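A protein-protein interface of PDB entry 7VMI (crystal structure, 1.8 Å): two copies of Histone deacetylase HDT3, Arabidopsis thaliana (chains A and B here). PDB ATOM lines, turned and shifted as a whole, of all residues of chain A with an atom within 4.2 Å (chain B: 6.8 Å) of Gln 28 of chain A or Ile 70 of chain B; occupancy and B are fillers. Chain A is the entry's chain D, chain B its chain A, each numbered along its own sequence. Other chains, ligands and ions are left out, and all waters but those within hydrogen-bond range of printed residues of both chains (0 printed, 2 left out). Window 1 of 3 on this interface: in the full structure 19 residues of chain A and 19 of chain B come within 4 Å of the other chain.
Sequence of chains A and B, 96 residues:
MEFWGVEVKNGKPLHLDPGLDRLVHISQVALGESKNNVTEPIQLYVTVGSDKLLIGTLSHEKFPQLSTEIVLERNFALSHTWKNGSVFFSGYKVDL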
ATOM      1  N   ILE A  26       2.587  22.381  17.960  1.00  0.00           N
ATOM      2  CA  ILE A  26       2.059  21.109  17.439  1.00  0.00           C
ATOM      3  C   ILE A  26       3.014  20.012  17.941  1.00  0.00           C
ATOM      4  O   ILE A  26       4.202  20.049  17.636  1.00  0.00           O
ATOM      5  CB  ILE A  26       1.987  21.061  15.919  1.00  0.00           C
ATOM      6  CG1 ILE A  26       1.121  22.211  15.415  1.00  0.00           C
ATOM      7  CG2 ILE A  26       1.413  19.744  15.457  1.00  0.00           C
ATOM      8  CD1 ILE A  26       0.987  22.340  13.909  1.00  0.00           C
ATOM      9  N   SER A  27       2.490  19.059  18.723  1.00  0.00           N
ATOM     10  CA  SER A  27       3.292  18.000  19.290  1.00  0.00           C
ATOM     11  C   SER A  27       3.040  16.607  18.713  1.00  0.00           C
ATOM     12  O   SER A  27       3.915  15.727  18.817  1.00  0.00           O
ATOM     13  CB  SER A  27       3.121  17.954  20.820  1.00  0.00           C
ATOM     14  OG  SER A  27       1.753  17.762  21.200  1.00  0.00           O
ATOM     15  N   GLN A  28       1.844  16.389  18.147  1.00  0.00           N
ATOM     16  CA  GLN A  28       1.431  15.063  17.678  1.00  0.00           C
ATOM     17  C   GLN A  28       0.710  15.104  16.376  1.00  0.00           C
ATOM     18  O   GLN A  28      -0.271  15.832  16.208  1.00  0.00           O
ATOM     19  CB  GLN A  28       0.571  14.332  18.720  1.00  0.00           C
ATOM     20  CG  GLN A  28       1.180  14.265  20.141  1.00  0.00           C
ATOM     21  CD  GLN A  28       2.529  13.550  20.264  1.00  0.00           C
ATOM     22  OE1 GLN A  28       3.324  13.890  21.134  1.00  0.00           O
ATOM     23  NE2 GLN A  28       2.770  12.526  19.444  1.00  0.00           N
ATOM     24  N   VAL A  29       1.171  14.266  15.450  1.00  0.00           N
ATOM     25  CA  VAL A  29       0.570  14.088  14.131  1.00  0.00           C
ATOM     26  C   VAL A  29       0.174  12.617  14.024  1.00  0.00           C
ATOM     27  O   VAL A  29       0.930  11.739  14.409  1.00  0.00           O
ATOM     28  CB  VAL A  29       1.585  14.459  13.047  1.00  0.00           C
ATOM     29  CG1 VAL A  29       0.985  14.304  11.668  1.00  0.00           C
ATOM     30  CG2 VAL A  29       2.027  15.889  13.229  1.00  0.00           C
ATOM     31  N   LEU A  66       3.672  10.921  14.050  1.00  0.00           N
ATOM     32  CA  LEU A  66       4.933  11.592  14.394  1.00  0.00           C
ATOM     33  C   LEU A  66       4.734  12.303  15.706  1.00  0.00           C
ATOM     34  O   LEU A  66       3.644  12.799  15.996  1.00  0.00           O
ATOM     35  CB  LEU A  66       5.310  12.662  13.376  1.00  0.00           C
ATOM     36  CG  LEU A  66       5.445  12.307  11.919  1.00  0.00           C
ATOM     37  CD1 LEU A  66       5.626  13.561  11.059  1.00  0.00           C
ATOM     38  CD2 LEU A  66       6.613  11.330  11.752  1.00  0.00           C
ATOM     39  N   SER A  67       5.817  12.391  16.461  1.00  0.00           N
ATOM     40  CA  SER A  67       5.904  13.215  17.660  1.00  0.00           C
ATOM     41  C   SER A  67       6.810  14.352  17.239  1.00  0.00           C
ATOM     42  O   SER A  67       7.944  14.133  16.757  1.00  0.00           O
ATOM     43  CB  SER A  67       6.473  12.408  18.805  1.00  0.00           C
ATOM     44  OG  SER A  67       5.518  11.443  19.233  1.00  0.00           O
ATOM     45  N   THR A  68       6.294  15.577  17.384  1.00  0.00           N
ATOM     46  CA  THR A  68       6.878  16.759  16.822  1.00  0.00           C
ATOM     47  C   THR A  68       7.034  17.870  17.852  1.00  0.00           C
ATOM     48  O   THR A  68       6.508  17.786  18.968  1.00  0.00           O
ATOM     49  CB  THR A  68       6.001  17.302  15.669  1.00  0.00           C
ATOM     50  OG1 THR A  68       4.706  17.669  16.150  1.00  0.00           O
ATOM     51  CG2 THR A  68       5.851  16.239  14.505  1.00  0.00           C
ATOM     52  N   PHE A  88      -4.523  14.120  11.598  1.00  0.00           N
ATOM     53  CA  PHE A  88      -4.866  14.801  12.835  1.00  0.00           C
ATOM     54  C   PHE A  88      -3.601  15.467  13.399  1.00  0.00           C
ATOM     55  O   PHE A  88      -2.554  14.855  13.485  1.00  0.00           O
ATOM     56  CB  PHE A  88      -5.429  13.817  13.844  1.00  0.00           C
ATOM     57  CG  PHE A  88      -6.776  13.268  13.461  1.00  0.00           C
ATOM     58  CD1 PHE A  88      -6.865  12.226  12.556  1.00  0.00           C
ATOM     59  CD2 PHE A  88      -7.941  13.762  14.041  1.00  0.00           C
ATOM     60  CE1 PHE A  88      -8.103  11.715  12.187  1.00  0.00           C
ATOM     61  CE2 PHE A  88      -9.190  13.259  13.659  1.00  0.00           C
ATOM     62  CZ  PHE A  88      -9.277  12.221  12.741  1.00  0.00           C
ATOM     63  N   PHE A  89      -3.714  16.748  13.752  1.00  0.00           N
ATOM     64  CA  PHE A  89      -2.629  17.489  14.359  1.00  0.00           C
ATOM     65  C   PHE A  89      -3.100  17.963  15.709  1.00  0.00           C
ATOM     66  O   PHE A  89      -4.186  18.526  15.825  1.00  0.00           O
ATOM     67  CB  PHE A  89      -2.287  18.712  13.511  1.00  0.00           C
ATOM     68  CG  PHE A  89      -1.805  18.405  12.140  1.00  0.00           C
ATOM     69  CD1 PHE A  89      -2.698  18.081  11.153  1.00  0.00           C
ATOM     70  CD2 PHE A  89      -0.468  18.491  11.819  1.00  0.00           C
ATOM     71  CE1 PHE A  89      -2.253  17.800   9.864  1.00  0.00           C
ATOM     72  CE2 PHE A  89      -0.018  18.211  10.537  1.00  0.00           C
ATOM     73  CZ  PHE A  89      -0.912  17.880   9.564  1.00  0.00           C
ATOM     74  N   SER A  90      -2.283  17.751  16.739  1.00  0.00           N
ATOM     75  CA  SER A  90      -2.623  18.198  18.079  1.00  0.00           C
ATOM     76  C   SER A  90      -1.436  18.739  18.853  1.00  0.00           C
ATOM     77  O   SER A  90      -0.289  18.515  18.518  1.00  0.00           O
ATOM     78  CB  SER A  90      -3.362  17.124  18.871  1.00  0.00           C
ATOM     79  OG  SER A  90      -2.613  15.961  19.110  1.00  0.00           O
ATOM     80  N   VAL B  24      -2.407  17.982  33.040  1.00  0.00           N
ATOM     81  CA  VAL B  24      -1.830  16.657  32.827  1.00  0.00           C
ATOM     82  C   VAL B  24      -0.966  16.734  31.570  1.00  0.00           C
ATOM     83  O   VAL B  24      -1.414  17.190  30.512  1.00  0.00           O
ATOM     84  CB  VAL B  24      -2.902  15.580  32.716  1.00  0.00           C
ATOM     85  CG1 VAL B  24      -2.270  14.274  32.329  1.00  0.00           C
ATOM     86  CG2 VAL B  24      -3.609  15.413  34.055  1.00  0.00           C
ATOM     87  N   HIS B  25       0.285  16.286  31.710  1.00  0.00           N
ATOM     88  CA  HIS B  25       1.265  16.148  30.630  1.00  0.00           C
ATOM     89  C   HIS B  25       1.470  14.660  30.382  1.00  0.00           C
ATOM     90  O   HIS B  25       1.999  13.958  31.256  1.00  0.00           O
ATOM     91  CB  HIS B  25       2.559  16.786  31.118  1.00  0.00           C
ATOM     92  CG  HIS B  25       3.591  16.955  30.071  1.00  0.00           C
ATOM     93  ND1 HIS B  25       4.163  15.926  29.331  1.00  0.00           N
ATOM     94  CD2 HIS B  25       4.221  18.087  29.681  1.00  0.00           C
ATOM     95  CE1 HIS B  25       5.079  16.431  28.516  1.00  0.00           C
ATOM     96  NE2 HIS B  25       5.132  17.740  28.705  1.00  0.00           N
ATOM     97  N   ILE B  26       0.974  14.156  29.241  1.00  0.00           N
ATOM     98  CA  ILE B  26       1.128  12.730  28.906  1.00  0.00           C
ATOM     99  C   ILE B  26       2.372  12.579  28.051  1.00  0.00           C
ATOM    100  O   ILE B  26       2.470  13.162  26.970  1.00  0.00           O
ATOM    101  CB  ILE B  26      -0.072  12.171  28.149  1.00  0.00           C
ATOM    102  CG1 ILE B  26      -1.345  12.381  28.962  1.00  0.00           C
ATOM    103  CG2 ILE B  26       0.125  10.663  27.820  1.00  0.00           C
ATOM    104  CD1 ILE B  26      -2.597  11.969  28.170  1.00  0.00           C
ATOM    105  N   SER B  27       3.339  11.803  28.550  1.00  0.00           N
ATOM    106  CA  SER B  27       4.628  11.632  27.866  1.00  0.00           C
ATOM    107  C   SER B  27       4.850  10.233  27.257  1.00  0.00           C
ATOM    108  O   SER B  27       5.654  10.096  26.339  1.00  0.00           O
ATOM    109  CB  SER B  27       5.778  11.971  28.812  1.00  0.00           C
ATOM    110  OG  SER B  27       5.763  11.169  29.991  1.00  0.00           O
ATOM    111  N   VAL B  29       3.001   6.392  26.092  1.00  0.00           N
ATOM    112  CA  VAL B  29       1.900   5.547  25.766  1.00  0.00           C
ATOM    113  C   VAL B  29       2.488   4.164  25.462  1.00  0.00           C
ATOM    114  O   VAL B  29       3.514   4.045  24.779  1.00  0.00           O
ATOM    115  CB  VAL B  29       1.160   6.084  24.552  1.00  0.00           C
ATOM    116  CG1 VAL B  29      -0.046   5.178  24.210  1.00  0.00           C
ATOM    117  CG2 VAL B  29       0.708   7.523  24.795  1.00  0.00           C
ATOM    118  N   VAL B  46      -7.793  11.156  22.212  1.00  0.00           N
ATOM    119  CA  VAL B  46      -8.003  12.053  23.335  1.00  0.00           C
ATOM    120  C   VAL B  46      -9.189  12.874  22.921  1.00  0.00           C
ATOM    121  O   VAL B  46      -9.202  13.432  21.811  1.00  0.00           O
ATOM    122  CB  VAL B  46      -6.809  13.003  23.546  1.00  0.00           C
ATOM    123  CG1 VAL B  46      -7.035  13.870  24.777  1.00  0.00           C
ATOM    124  CG2 VAL B  46      -5.531  12.258  23.681  1.00  0.00           C
ATOM    125  N   LEU B  54      -7.413  11.759  17.069  1.00  0.00           N
ATOM    126  CA  LEU B  54      -6.532  10.619  16.912  1.00  0.00           C
ATOM    127  C   LEU B  54      -5.122  11.064  17.268  1.00  0.00           C
ATOM    128  O   LEU B  54      -4.617  12.067  16.708  1.00  0.00           O
ATOM    129  CB  LEU B  54      -6.573  10.129  15.461  1.00  0.00           C
ATOM    130  CG  LEU B  54      -5.725   8.871  15.183  1.00  0.00           C
ATOM    131  CD1 LEU B  54      -6.300   7.625  15.860  1.00  0.00           C
ATOM    132  CD2 LEU B  54      -5.514   8.679  13.692  1.00  0.00           C
ATOM    133  N   ILE B  55      -4.487  10.355  18.206  1.00  0.00           N
ATOM    134  CA  ILE B  55      -3.102  10.599  18.526  1.00  0.00           C
ATOM    135  C   ILE B  55      -2.130   9.553  17.999  1.00  0.00           C
ATOM    136  O   ILE B  55      -0.923   9.804  17.954  1.00  0.00           O
ATOM    137  CB  ILE B  55      -2.882  10.827  20.033  1.00  0.00           C
ATOM    138  CG1 ILE B  55      -3.231   9.604  20.831  1.00  0.00           C
ATOM    139  CG2 ILE B  55      -3.646  12.045  20.537  1.00  0.00           C
ATOM    140  CD1 ILE B  55      -2.917   9.766  22.277  1.00  0.00           C
ATOM    141  N   LEU B  66       4.560   4.854  22.228  1.00  0.00           N
ATOM    142  CA  LEU B  66       4.822   6.190  21.704  1.00  0.00           C
ATOM    143  C   LEU B  66       5.404   7.026  22.817  1.00  0.00           C
ATOM    144  O   LEU B  66       5.012   6.872  23.999  1.00  0.00           O
ATOM    145  CB  LEU B  66       3.529   6.882  21.298  1.00  0.00           C
ATOM    146  CG  LEU B  66       2.684   6.246  20.196  1.00  0.00           C
ATOM    147  CD1 LEU B  66       1.396   6.996  19.941  1.00  0.00           C
ATOM    148  CD2 LEU B  66       3.436   6.148  18.885  1.00  0.00           C
ATOM    149  N   SER B  67       6.307   7.929  22.431  1.00  0.00           N
ATOM    150  CA  SER B  67       6.801   8.964  23.282  1.00  0.00           C
ATOM    151  C   SER B  67       6.161  10.235  22.798  1.00  0.00           C
ATOM    152  O   SER B  67       6.290  10.578  21.615  1.00  0.00           O
ATOM    153  CB  SER B  67       8.343   8.989  23.234  1.00  0.00           C
ATOM    154  OG  SER B  67       8.861   7.837  23.878  1.00  0.00           O
ATOM    155  N   THR B  68       5.449  10.910  23.702  1.00  0.00           N
ATOM    156  CA  THR B  68       4.510  11.965  23.344  1.00  0.00           C
ATOM    157  C   THR B  68       4.735  13.219  24.192  1.00  0.00           C
ATOM    158  O   THR B  68       5.488  13.195  25.168  1.00  0.00           O
ATOM    159  CB  THR B  68       3.039  11.506  23.557  1.00  0.00           C
ATOM    160  OG1 THR B  68       2.814  11.188  24.966  1.00  0.00           O
ATOM    161  CG2 THR B  68       2.703  10.331  22.672  1.00  0.00           C
ATOM    162  N   GLU B  69       4.042  14.288  23.798  1.00  0.00           N
ATOM    163  CA  GLU B  69       3.953  15.501  24.610  1.00  0.00           C
ATOM    164  C   GLU B  69       2.554  16.082  24.462  1.00  0.00           C
ATOM    165  O   GLU B  69       2.323  16.987  23.665  1.00  0.00           O
ATOM    166  CB  GLU B  69       5.072  16.481  24.246  1.00  0.00           C
ATOM    167  CG  GLU B  69       5.076  17.700  25.163  1.00  0.00           C
ATOM    168  CD  GLU B  69       6.273  18.598  24.960  1.00  0.00           C
ATOM    169  OE1 GLU B  69       7.391  18.127  24.639  1.00  0.00           O
ATOM    170  OE2 GLU B  69       6.096  19.819  24.995  1.00  0.00           O
ATOM    171  N   ILE B  70       1.613  15.507  25.221  1.00  0.00           N
ATOM    172  CA  ILE B  70       0.204  15.873  25.175  1.00  0.00           C
ATOM    173  C   ILE B  70      -0.123  16.627  26.466  1.00  0.00           C
ATOM    174  O   ILE B  70       0.161  16.133  27.554  1.00  0.00           O
ATOM    175  CB  ILE B  70      -0.648  14.643  25.039  1.00  0.00           C
ATOM    176  CG1 ILE B  70      -0.266  13.879  23.763  1.00  0.00           C
ATOM    177  CG2 ILE B  70      -2.119  15.003  24.981  1.00  0.00           C
ATOM    178  CD1 ILE B  70      -0.854  12.483  23.777  1.00  0.00           C
ATOM    179  N   VAL B  71      -0.673  17.833  26.321  1.00  0.00           N
ATOM    180  CA  VAL B  71      -0.870  18.758  27.426  1.00  0.00           C
ATOM    181  C   VAL B  71      -2.365  19.113  27.561  1.00  0.00           C
ATOM    182  O   VAL B  71      -2.960  19.632  26.652  1.00  0.00           O
ATOM    183  CB  VAL B  71       0.012  19.989  27.266  1.00  0.00           C
ATOM    184  CG1 VAL B  71      -0.314  21.068  28.306  1.00  0.00           C
ATOM    185  CG2 VAL B  71       1.484  19.572  27.399  1.00  0.00           C
ATOM    186  N   LEU B  72      -2.936  18.811  28.738  1.00  0.00           N
ATOM    187  CA  LEU B  72      -4.361  18.880  28.988  1.00  0.00           C
ATOM    188  C   LEU B  72      -4.648  19.695  30.242  1.00  0.00           C
ATOM    189  O   LEU B  72      -4.213  19.346  31.349  1.00  0.00           O
ATOM    190  CB  LEU B  72      -4.881  17.466  29.138  1.00  0.00           C
ATOM    191  CG  LEU B  72      -4.709  16.684  27.836  1.00  0.00           C
ATOM    192  CD1 LEU B  72      -4.527  15.215  28.149  1.00  0.00           C
ATOM    193  CD2 LEU B  72      -5.865  16.937  26.856  1.00  0.00           C
ATOM    194  N   LEU B  78      -9.601   9.552  27.561  1.00  0.00           N
ATOM    195  CA  LEU B  78      -8.730   8.689  26.790  1.00  0.00           C
ATOM    196  C   LEU B  78      -9.502   7.450  26.406  1.00  0.00           C
ATOM    197  O   LEU B  78     -10.258   6.888  27.197  1.00  0.00           O
ATOM    198  CB  LEU B  78      -7.498   8.322  27.611  1.00  0.00           C
ATOM    199  CG  LEU B  78      -6.641   9.490  28.091  1.00  0.00           C
ATOM    200  CD1 LEU B  78      -5.531   9.039  29.015  1.00  0.00           C
ATOM    201  CD2 LEU B  78      -6.029  10.252  26.926  1.00  0.00           C
ATOM    202  N   PHE B  89      -1.134   4.973  29.788  1.00  0.00           N
ATOM    203  CA  PHE B  89      -0.752   6.341  29.553  1.00  0.00           C
ATOM    204  C   PHE B  89      -0.104   6.854  30.815  1.00  0.00           C
ATOM    205  O   PHE B  89      -0.663   6.702  31.902  1.00  0.00           O
ATOM    206  CB  PHE B  89      -1.963   7.216  29.254  1.00  0.00           C
ATOM    207  CG  PHE B  89      -2.726   6.827  28.036  1.00  0.00           C
ATOM    208  CD1 PHE B  89      -3.616   5.768  28.090  1.00  0.00           C
ATOM    209  CD2 PHE B  89      -2.591   7.543  26.859  1.00  0.00           C
ATOM    210  CE1 PHE B  89      -4.343   5.404  26.973  1.00  0.00           C
ATOM    211  CE2 PHE B  89      -3.306   7.198  25.738  1.00  0.00           C
ATOM    212  CZ  PHE B  89      -4.205   6.139  25.794  1.00  0.00           C
ATOM    213  N   TYR B  92       2.929  13.224  33.951  1.00  0.00           N
ATOM    214  CA  TYR B  92       2.999  14.009  35.201  1.00  0.00           C
ATOM    215  C   TYR B  92       2.000  15.169  35.191  1.00  0.00           C
ATOM    216  O   TYR B  92       1.615  15.660  34.116  1.00  0.00           O
ATOM    217  CB  TYR B  92       4.437  14.475  35.451  1.00  0.00           C
ATOM    218  CG  TYR B  92       5.097  15.209  34.305  1.00  0.00           C
ATOM    219  CD1 TYR B  92       5.817  14.546  33.329  1.00  0.00           C
ATOM    220  CD2 TYR B  92       5.025  16.587  34.213  1.00  0.00           C
ATOM    221  CE1 TYR B  92       6.424  15.220  32.286  1.00  0.00           C
ATOM    222  CE2 TYR B  92       5.628  17.280  33.170  1.00  0.00           C
ATOM    223  CZ  TYR B  92       6.346  16.592  32.220  1.00  0.00           C
ATOM    224  OH  TYR B  92       6.948  17.268  31.202  1.00  0.00           O
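The backbone carbonyl oxygen (O) of Ser 67 of chain B sits at hydrogen-bond distance from the side-chain hydroxyl (OG) of Ser 67 of chain A, 2.6 Å away. OE1 of Gln 28 of chain A is in hydrogen-bond range of N of Glu 69 of chain B (2.8 Å). The side-chain hydroxyl (OG) of Ser 27 of chain A sits at hydrogen-bond distance from the backbone carbonyl oxygen (O) of Glu 69 of chain B (2.6 Å).
Ser 67 of chain A touches its own counterpart, Ser 67 of chain B. Positions printed for both chains: 26, 27, 29, 66, 67, 68 and 89. Of the 6 pairs that touch across the chains among the printed residues, 1 has its exchanged pair printed and touching as well.
The backbone carbonyl oxygen of Ile 26 of chain B sits at hydrogen-bond distance from the side-chain hydroxyl of Thr 68 of chain B (2.8 Å). O of Ser 27 of chain A is in hydrogen-bond range of N of Thr 68 of chain A (2.8 Å). The backbone carbonyl oxygen of Gln 28 of chain A lies within hydrogen-bond range of the backbone NH of Ser 90 of chain A (2.8 Å). O of Ile 70 of chain B lies within hydrogen-bond range of N of Ile 26 of chain B (2.7 Å). The backbone NH of Thr 68 of chain B is in hydrogen-bond range of the backbone carbonyl oxygen of Ser 27 of chain B (2.8 Å). OG of Ser 67 of chain A sits at hydrogen-bond distance from NE2 of Gln 28 of chain A.
Among the printed residues, pairs that only touch across the chains: Gln 28 of chain A with Thr 68 of chain B (3.2 Å), Gln 28 of chain A with Ile 70 of chain B (3.9 Å) and Phe 88 of chain A with Leu 54 of chain B (3.5 Å).
Of the 18 printed residues of chain B, 5 touch a printed residue of chain A. Printed residues of chain B that touch a printed residue of chain A: Leu 54, Ser 67, Thr 68, Glu 69 and Ile 70. Of the 10 printed residues of chain A, 4 touch a printed residue of chain B. Hydrophobic or aromatic side chains of chain A within 4 Å of the printed part of chain B: Phe 88.
Printed residues of chain B within 4 Å of Phe 88 of chain A: Leu 54 (3.5 Å). Of the printed residues of chain B, Ser 27 of chain A touches Glu 69. Of the printed residues of chain A, Leu 54 of chain B touches Phe 88. The nearest printed residue of chain A that does not touch Leu 54 of chain B is Ser 90 of chain A (5.0 Å).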
